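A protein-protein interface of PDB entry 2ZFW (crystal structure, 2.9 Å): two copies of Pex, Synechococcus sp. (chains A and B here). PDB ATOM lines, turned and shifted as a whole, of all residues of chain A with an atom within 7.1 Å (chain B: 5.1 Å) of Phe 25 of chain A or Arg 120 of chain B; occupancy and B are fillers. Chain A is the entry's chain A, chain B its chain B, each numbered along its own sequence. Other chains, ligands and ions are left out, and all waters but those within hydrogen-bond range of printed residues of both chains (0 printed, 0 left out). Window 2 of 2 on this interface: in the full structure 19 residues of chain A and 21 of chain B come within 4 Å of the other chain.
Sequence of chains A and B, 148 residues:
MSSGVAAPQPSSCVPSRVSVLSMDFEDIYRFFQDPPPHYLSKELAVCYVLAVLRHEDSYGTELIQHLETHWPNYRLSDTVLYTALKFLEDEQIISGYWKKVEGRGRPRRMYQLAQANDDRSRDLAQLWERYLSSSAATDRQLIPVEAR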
ATOM      1  N   MET A  23     -16.121  22.384   9.914  1.00  0.00           N
ATOM      2  CA  MET A  23     -16.313  21.439   8.773  1.00  0.00           C
ATOM      3  C   MET A  23     -17.767  21.409   8.321  1.00  0.00           C
ATOM      4  O   MET A  23     -18.688  21.410   9.140  1.00  0.00           O
ATOM      5  CB  MET A  23     -15.891  20.017   9.170  1.00  0.00           C
ATOM      6  CG  MET A  23     -16.802  19.354  10.207  1.00  0.00           C
ATOM      7  SD  MET A  23     -16.276  17.694  10.718  1.00  0.00           S
ATOM      8  CE  MET A  23     -17.173  17.527  12.286  1.00  0.00           C
ATOM      9  N   ASP A  24     -17.959  21.376   7.011  1.00  0.00           N
ATOM     10  CA  ASP A  24     -19.287  21.333   6.442  1.00  0.00           C
ATOM     11  C   ASP A  24     -19.572  19.892   6.007  1.00  0.00           C
ATOM     12  O   ASP A  24     -18.663  19.071   5.976  1.00  0.00           O
ATOM     13  CB  ASP A  24     -19.366  22.270   5.236  1.00  0.00           C
ATOM     14  CG  ASP A  24     -20.773  22.382   4.692  1.00  0.00           C
ATOM     15  OD1 ASP A  24     -20.936  22.560   3.466  1.00  0.00           O
ATOM     16  OD2 ASP A  24     -21.717  22.291   5.508  1.00  0.00           O
ATOM     17  N   PHE A  25     -20.821  19.591   5.660  1.00  0.00           N
ATOM     18  CA  PHE A  25     -21.188  18.248   5.229  1.00  0.00           C
ATOM     19  C   PHE A  25     -20.500  17.750   3.962  1.00  0.00           C
ATOM     20  O   PHE A  25     -20.476  16.555   3.715  1.00  0.00           O
ATOM     21  CB  PHE A  25     -22.699  18.135   5.054  1.00  0.00           C
ATOM     22  CG  PHE A  25     -23.453  18.091   6.349  1.00  0.00           C
ATOM     23  CD1 PHE A  25     -24.040  19.242   6.872  1.00  0.00           C
ATOM     24  CD2 PHE A  25     -23.546  16.903   7.072  1.00  0.00           C
ATOM     25  CE1 PHE A  25     -24.719  19.209   8.099  1.00  0.00           C
ATOM     26  CE2 PHE A  25     -24.217  16.858   8.292  1.00  0.00           C
ATOM     27  CZ  PHE A  25     -24.803  18.019   8.808  1.00  0.00           C
ATOM     28  N   GLU A  26     -19.953  18.646   3.150  1.00  0.00           N
ATOM     29  CA  GLU A  26     -19.263  18.210   1.943  1.00  0.00           C
ATOM     30  C   GLU A  26     -17.848  17.788   2.324  1.00  0.00           C
ATOM     31  O   GLU A  26     -17.130  17.154   1.553  1.00  0.00           O
ATOM     32  CB  GLU A  26     -19.206  19.337   0.908  1.00  0.00           C
ATOM     33  CG  GLU A  26     -18.628  20.636   1.432  1.00  0.00           C
ATOM     34  CD  GLU A  26     -17.908  21.445   0.354  1.00  0.00           C
ATOM     35  OE1 GLU A  26     -18.450  21.571  -0.765  1.00  0.00           O
ATOM     36  OE2 GLU A  26     -16.801  21.964   0.631  1.00  0.00           O
ATOM     37  N   ASP A  27     -17.443  18.163   3.527  1.00  0.00           N
ATOM     38  CA  ASP A  27     -16.120  17.816   4.019  1.00  0.00           C
ATOM     39  C   ASP A  27     -16.152  16.372   4.508  1.00  0.00           C
ATOM     40  O   ASP A  27     -15.260  15.581   4.196  1.00  0.00           O
ATOM     41  CB  ASP A  27     -15.735  18.746   5.169  1.00  0.00           C
ATOM     42  CG  ASP A  27     -15.415  20.148   4.701  1.00  0.00           C
ATOM     43  OD1 ASP A  27     -14.274  20.362   4.245  1.00  0.00           O
ATOM     44  OD2 ASP A  27     -16.300  21.030   4.782  1.00  0.00           O
ATOM     45  N   ILE A  28     -17.196  16.039   5.263  1.00  0.00           N
ATOM     46  CA  ILE A  28     -17.359  14.698   5.809  1.00  0.00           C
ATOM     47  C   ILE A  28     -17.454  13.645   4.715  1.00  0.00           C
ATOM     48  O   ILE A  28     -16.827  12.591   4.820  1.00  0.00           O
ATOM     49  CB  ILE A  28     -18.605  14.606   6.696  1.00  0.00           C
ATOM     50  CG1 ILE A  28     -18.453  15.552   7.888  1.00  0.00           C
ATOM     51  CG2 ILE A  28     -18.790  13.185   7.197  1.00  0.00           C
ATOM     52  CD1 ILE A  28     -19.687  15.629   8.762  1.00  0.00           C
ATOM     53  N   TYR A  29     -18.226  13.919   3.667  1.00  0.00           N
ATOM     54  CA  TYR A  29     -18.347  12.956   2.577  1.00  0.00           C
ATOM     55  C   TYR A  29     -17.050  12.888   1.780  1.00  0.00           C
ATOM     56  O   TYR A  29     -16.535  11.799   1.513  1.00  0.00           O
ATOM     57  CB  TYR A  29     -19.523  13.303   1.660  1.00  0.00           C
ATOM     58  CG  TYR A  29     -20.876  12.911   2.232  1.00  0.00           C
ATOM     59  CD1 TYR A  29     -21.440  13.619   3.295  1.00  0.00           C
ATOM     60  CD2 TYR A  29     -21.578  11.822   1.719  1.00  0.00           C
ATOM     61  CE1 TYR A  29     -22.673  13.255   3.836  1.00  0.00           C
ATOM     62  CE2 TYR A  29     -22.808  11.443   2.246  1.00  0.00           C
ATOM     63  CZ  TYR A  29     -23.353  12.165   3.309  1.00  0.00           C
ATOM     64  OH  TYR A  29     -24.569  11.796   3.850  1.00  0.00           O
ATOM     65  N   ARG A  30     -16.506  14.050   1.432  1.00  0.00           N
ATOM     66  CA  ARG A  30     -15.269  14.115   0.662  1.00  0.00           C
ATOM     67  C   ARG A  30     -14.103  13.599   1.491  1.00  0.00           C
ATOM     68  O   ARG A  30     -12.943  13.869   1.172  1.00  0.00           O
ATOM     69  CB  ARG A  30     -14.998  15.559   0.223  1.00  0.00           C
ATOM     70  CG  ARG A  30     -14.000  15.676  -0.916  1.00  0.00           C
ATOM     71  CD  ARG A  30     -13.845  17.105  -1.446  1.00  0.00           C
ATOM     72  NE  ARG A  30     -13.099  17.990  -0.547  1.00  0.00           N
ATOM     73  CZ  ARG A  30     -13.629  18.659   0.477  1.00  0.00           C
ATOM     74  NH1 ARG A  30     -14.930  18.557   0.750  1.00  0.00           N
ATOM     75  NH2 ARG A  30     -12.860  19.435   1.234  1.00  0.00           N
ATOM     76  N   LEU B  50     -23.028   9.309  15.484  1.00  0.00           N
ATOM     77  CA  LEU B  50     -24.362   9.267  14.898  1.00  0.00           C
ATOM     78  C   LEU B  50     -24.887   7.852  14.848  1.00  0.00           C
ATOM     79  O   LEU B  50     -26.055   7.631  15.145  1.00  0.00           O
ATOM     80  CB  LEU B  50     -24.373   9.905  13.502  1.00  0.00           C
ATOM     81  CG  LEU B  50     -24.718  11.391  13.593  1.00  0.00           C
ATOM     82  CD1 LEU B  50     -24.434  12.097  12.293  1.00  0.00           C
ATOM     83  CD2 LEU B  50     -26.172  11.520  13.980  1.00  0.00           C
ATOM     84  N   PHE B  87     -20.585  20.148  16.080  1.00  0.00           N
ATOM     85  CA  PHE B  87     -21.017  20.138  14.695  1.00  0.00           C
ATOM     86  C   PHE B  87     -22.435  19.603  14.606  1.00  0.00           C
ATOM     87  O   PHE B  87     -23.300  20.239  14.007  1.00  0.00           O
ATOM     88  CB  PHE B  87     -20.097  19.262  13.841  1.00  0.00           C
ATOM     89  CG  PHE B  87     -20.600  19.054  12.439  1.00  0.00           C
ATOM     90  CD1 PHE B  87     -20.478  20.057  11.489  1.00  0.00           C
ATOM     91  CD2 PHE B  87     -21.273  17.880  12.094  1.00  0.00           C
ATOM     92  CE1 PHE B  87     -21.025  19.898  10.220  1.00  0.00           C
ATOM     93  CE2 PHE B  87     -21.821  17.717  10.831  1.00  0.00           C
ATOM     94  CZ  PHE B  87     -21.697  18.729   9.893  1.00  0.00           C
ATOM     95  N   GLU B  91     -25.757  21.914  13.685  1.00  0.00           N
ATOM     96  CA  GLU B  91     -26.517  21.629  12.470  1.00  0.00           C
ATOM     97  C   GLU B  91     -27.899  21.130  12.846  1.00  0.00           C
ATOM     98  O   GLU B  91     -28.718  20.804  11.988  1.00  0.00           O
ATOM     99  CB  GLU B  91     -25.796  20.594  11.606  1.00  0.00           C
ATOM    100  CG  GLU B  91     -24.358  20.973  11.239  1.00  0.00           C
ATOM    101  CD  GLU B  91     -24.233  22.370  10.667  1.00  0.00           C
ATOM    102  OE1 GLU B  91     -24.996  22.704   9.744  1.00  0.00           O
ATOM    103  OE2 GLU B  91     -23.365  23.133  11.138  1.00  0.00           O
ATOM    104  N   GLN B  92     -28.153  21.084  14.147  1.00  0.00           N
ATOM    105  CA  GLN B  92     -29.438  20.653  14.674  1.00  0.00           C
ATOM    106  C   GLN B  92     -29.827  19.230  14.273  1.00  0.00           C
ATOM    107  O   GLN B  92     -30.917  19.000  13.755  1.00  0.00           O
ATOM    108  CB  GLN B  92     -30.531  21.639  14.244  1.00  0.00           C
ATOM    109  CG  GLN B  92     -30.149  23.112  14.468  1.00  0.00           C
ATOM    110  CD  GLN B  92     -31.274  24.078  14.123  1.00  0.00           C
ATOM    111  OE1 GLN B  92     -31.913  23.965  13.070  1.00  0.00           O
ATOM    112  NE2 GLN B  92     -31.516  25.041  15.009  1.00  0.00           N
ATOM    113  N   ILE B  93     -28.930  18.277  14.513  1.00  0.00           N
ATOM    114  CA  ILE B  93     -29.191  16.868  14.212  1.00  0.00           C
ATOM    115  C   ILE B  93     -29.265  16.095  15.525  1.00  0.00           C
ATOM    116  O   ILE B  93     -29.871  15.032  15.596  1.00  0.00           O
ATOM    117  CB  ILE B  93     -28.090  16.270  13.321  1.00  0.00           C
ATOM    118  CG1 ILE B  93     -28.137  16.935  11.950  1.00  0.00           C
ATOM    119  CG2 ILE B  93     -28.294  14.777  13.154  1.00  0.00           C
ATOM    120  CD1 ILE B  93     -26.971  16.588  11.069  1.00  0.00           C
ATOM    121  N   ASP B 118     -35.407  11.292  10.711  1.00  0.00           N
ATOM    122  CA  ASP B 118     -34.274  12.040  10.188  1.00  0.00           C
ATOM    123  C   ASP B 118     -33.563  11.153   9.165  1.00  0.00           C
ATOM    124  O   ASP B 118     -33.489   9.936   9.334  1.00  0.00           O
ATOM    125  CB  ASP B 118     -33.333  12.405  11.351  1.00  0.00           C
ATOM    126  CG  ASP B 118     -32.544  13.681  11.102  1.00  0.00           C
ATOM    127  OD1 ASP B 118     -33.131  14.662  10.604  1.00  0.00           O
ATOM    128  OD2 ASP B 118     -31.337  13.705  11.424  1.00  0.00           O
ATOM    129  N   ASP B 119     -33.074  11.761   8.090  1.00  0.00           N
ATOM    130  CA  ASP B 119     -32.358  11.012   7.067  1.00  0.00           C
ATOM    131  C   ASP B 119     -30.885  11.407   6.980  1.00  0.00           C
ATOM    132  O   ASP B 119     -30.063  10.632   6.504  1.00  0.00           O
ATOM    133  CB  ASP B 119     -33.030  11.167   5.692  1.00  0.00           C
ATOM    134  CG  ASP B 119     -34.012  10.035   5.383  1.00  0.00           C
ATOM    135  OD1 ASP B 119     -35.199  10.336   5.132  1.00  0.00           O
ATOM    136  OD2 ASP B 119     -33.599   8.850   5.391  1.00  0.00           O
ATOM    137  N   ARG B 120     -30.551  12.611   7.435  1.00  0.00           N
ATOM    138  CA  ARG B 120     -29.162  13.053   7.416  1.00  0.00           C
ATOM    139  C   ARG B 120     -28.338  12.181   8.368  1.00  0.00           C
ATOM    140  O   ARG B 120     -27.166  11.905   8.113  1.00  0.00           O
ATOM    141  CB  ARG B 120     -29.041  14.529   7.830  1.00  0.00           C
ATOM    142  CG  ARG B 120     -28.737  15.498   6.684  1.00  0.00           C
ATOM    143  CD  ARG B 120     -28.284  16.866   7.209  1.00  0.00           C
ATOM    144  NE  ARG B 120     -29.174  17.388   8.250  1.00  0.00           N
ATOM    145  CZ  ARG B 120     -28.981  18.529   8.913  1.00  0.00           C
ATOM    146  NH1 ARG B 120     -27.920  19.287   8.648  1.00  0.00           N
ATOM    147  NH2 ARG B 120     -29.856  18.917   9.836  1.00  0.00           N
ATOM    148  N   SER B 121     -28.948  11.752   9.469  1.00  0.00           N
ATOM    149  CA  SER B 121     -28.250  10.893  10.416  1.00  0.00           C
ATOM    150  C   SER B 121     -28.065   9.503   9.803  1.00  0.00           C
ATOM    151  O   SER B 121     -26.943   9.032   9.655  1.00  0.00           O
ATOM    152  CB  SER B 121     -29.016  10.810  11.741  1.00  0.00           C
ATOM    153  OG  SER B 121     -30.403  10.725  11.535  1.00  0.00           O
ATOM    154  N   ARG B 122     -29.163   8.857   9.427  1.00  0.00           N
ATOM    155  CA  ARG B 122     -29.110   7.526   8.814  1.00  0.00           C
ATOM    156  C   ARG B 122     -27.940   7.420   7.836  1.00  0.00           C
ATOM    157  O   ARG B 122     -27.042   6.594   7.998  1.00  0.00           O
ATOM    158  CB  ARG B 122     -30.428   7.254   8.073  1.00  0.00           C
ATOM    159  CG  ARG B 122     -30.713   5.789   7.733  1.00  0.00           C
ATOM    160  CD  ARG B 122     -32.221   5.572   7.428  1.00  0.00           C
ATOM    161  NE  ARG B 122     -33.097   6.095   8.489  1.00  0.00           N
ATOM    162  CZ  ARG B 122     -34.432   6.083   8.468  1.00  0.00           C
ATOM    163  NH1 ARG B 122     -35.089   5.569   7.434  1.00  0.00           N
ATOM    164  NH2 ARG B 122     -35.111   6.599   9.489  1.00  0.00           N
ATOM    165  N   ASP B 123     -27.965   8.269   6.818  1.00  0.00           N
ATOM    166  CA  ASP B 123     -26.933   8.269   5.793  1.00  0.00           C
ATOM    167  C   ASP B 123     -25.552   8.432   6.370  1.00  0.00           C
ATOM    168  O   ASP B 123     -24.605   7.774   5.952  1.00  0.00           O
ATOM    169  CB  ASP B 123     -27.210   9.367   4.761  1.00  0.00           C
ATOM    170  CG  ASP B 123     -28.187   8.914   3.699  1.00  0.00           C
ATOM    171  OD1 ASP B 123     -29.355   8.625   4.046  1.00  0.00           O
ATOM    172  OD2 ASP B 123     -27.779   8.826   2.521  1.00  0.00           O
ATOM    173  N   LEU B 124     -25.421   9.286   7.356  1.00  0.00           N
ATOM    174  CA  LEU B 124     -24.104   9.464   7.897  1.00  0.00           C
ATOM    175  C   LEU B 124     -23.633   8.298   8.746  1.00  0.00           C
ATOM    176  O   LEU B 124     -22.437   8.042   8.835  1.00  0.00           O
ATOM    177  CB  LEU B 124     -24.056  10.773   8.657  1.00  0.00           C
ATOM    178  CG  LEU B 124     -23.928  11.961   7.714  1.00  0.00           C
ATOM    179  CD1 LEU B 124     -24.301  13.222   8.455  1.00  0.00           C
ATOM    180  CD2 LEU B 124     -22.506  12.029   7.193  1.00  0.00           C
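Of the printed residues of chain B, Met 23 of chain A touches Phe 87.
Asp 24 of chain A touches none of the printed residues of chain B.
Phe 25 of chain A touches just these residues of chain B: Phe 87 (3.4 Å), Glu 91 (3.6 Å), Ile 93 (3.4 Å), Arg 120 (3.2 Å) and Leu 124 (3.6 Å).
Of the printed residues of chain A, Ile 93 of chain B touches Phe 25 (3.4 Å).
Ser 121 of chain B touches none of the printed residues of chain A.
Printed residues of chain A within 4 Å of Leu 124 of chain B: Phe 25, Ile 28 and Tyr 29.
The nearest residue of chain A that does not touch Arg 120 of chain B is Tyr 29 of chain A (5.0 Å).
O of Glu 91 of chain B is in hydrogen-bond range of NH2 of Arg 120 of chain B (3.1 Å).
Met 23 of chain A touches Phe 87 of chain B.
CZ of Phe 87 of chain B touches CZ of Phe 25 of chain A, 3.4 Å away.
CE1 of Phe 25 of chain A touches CG of Glu 91 of chain B, at 3.6 Å.
Phe 25 of chain A touches Ile 93 of chain B.
NH1 of Arg 120 of chain B touches CE1 of Phe 25 of chain A, 3.2 Å away.
Phe 25 of chain A touches Leu 124 of chain B (CE2 to CD1, 3.6 Å).
Ile 28 of chain A touches Phe 87 of chain B.
CG2 of Ile 28 of chain A touches CD2 of Leu 124 of chain B (3.9 Å).
Tyr 29 of chain A touches Asp 123 of chain B (OH to CB, 3.7 Å).
Tyr 29 of chain A touches Leu 124 of chain B.
No position is printed for both chains.
Of the 10 pairs that touch across the chains among the printed residues, none has its exchanged pair printed and touching as well.
Printed residues of chain A that touch a printed residue of chain B: Met 23, Phe 25, Ile 28 and Tyr 29.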
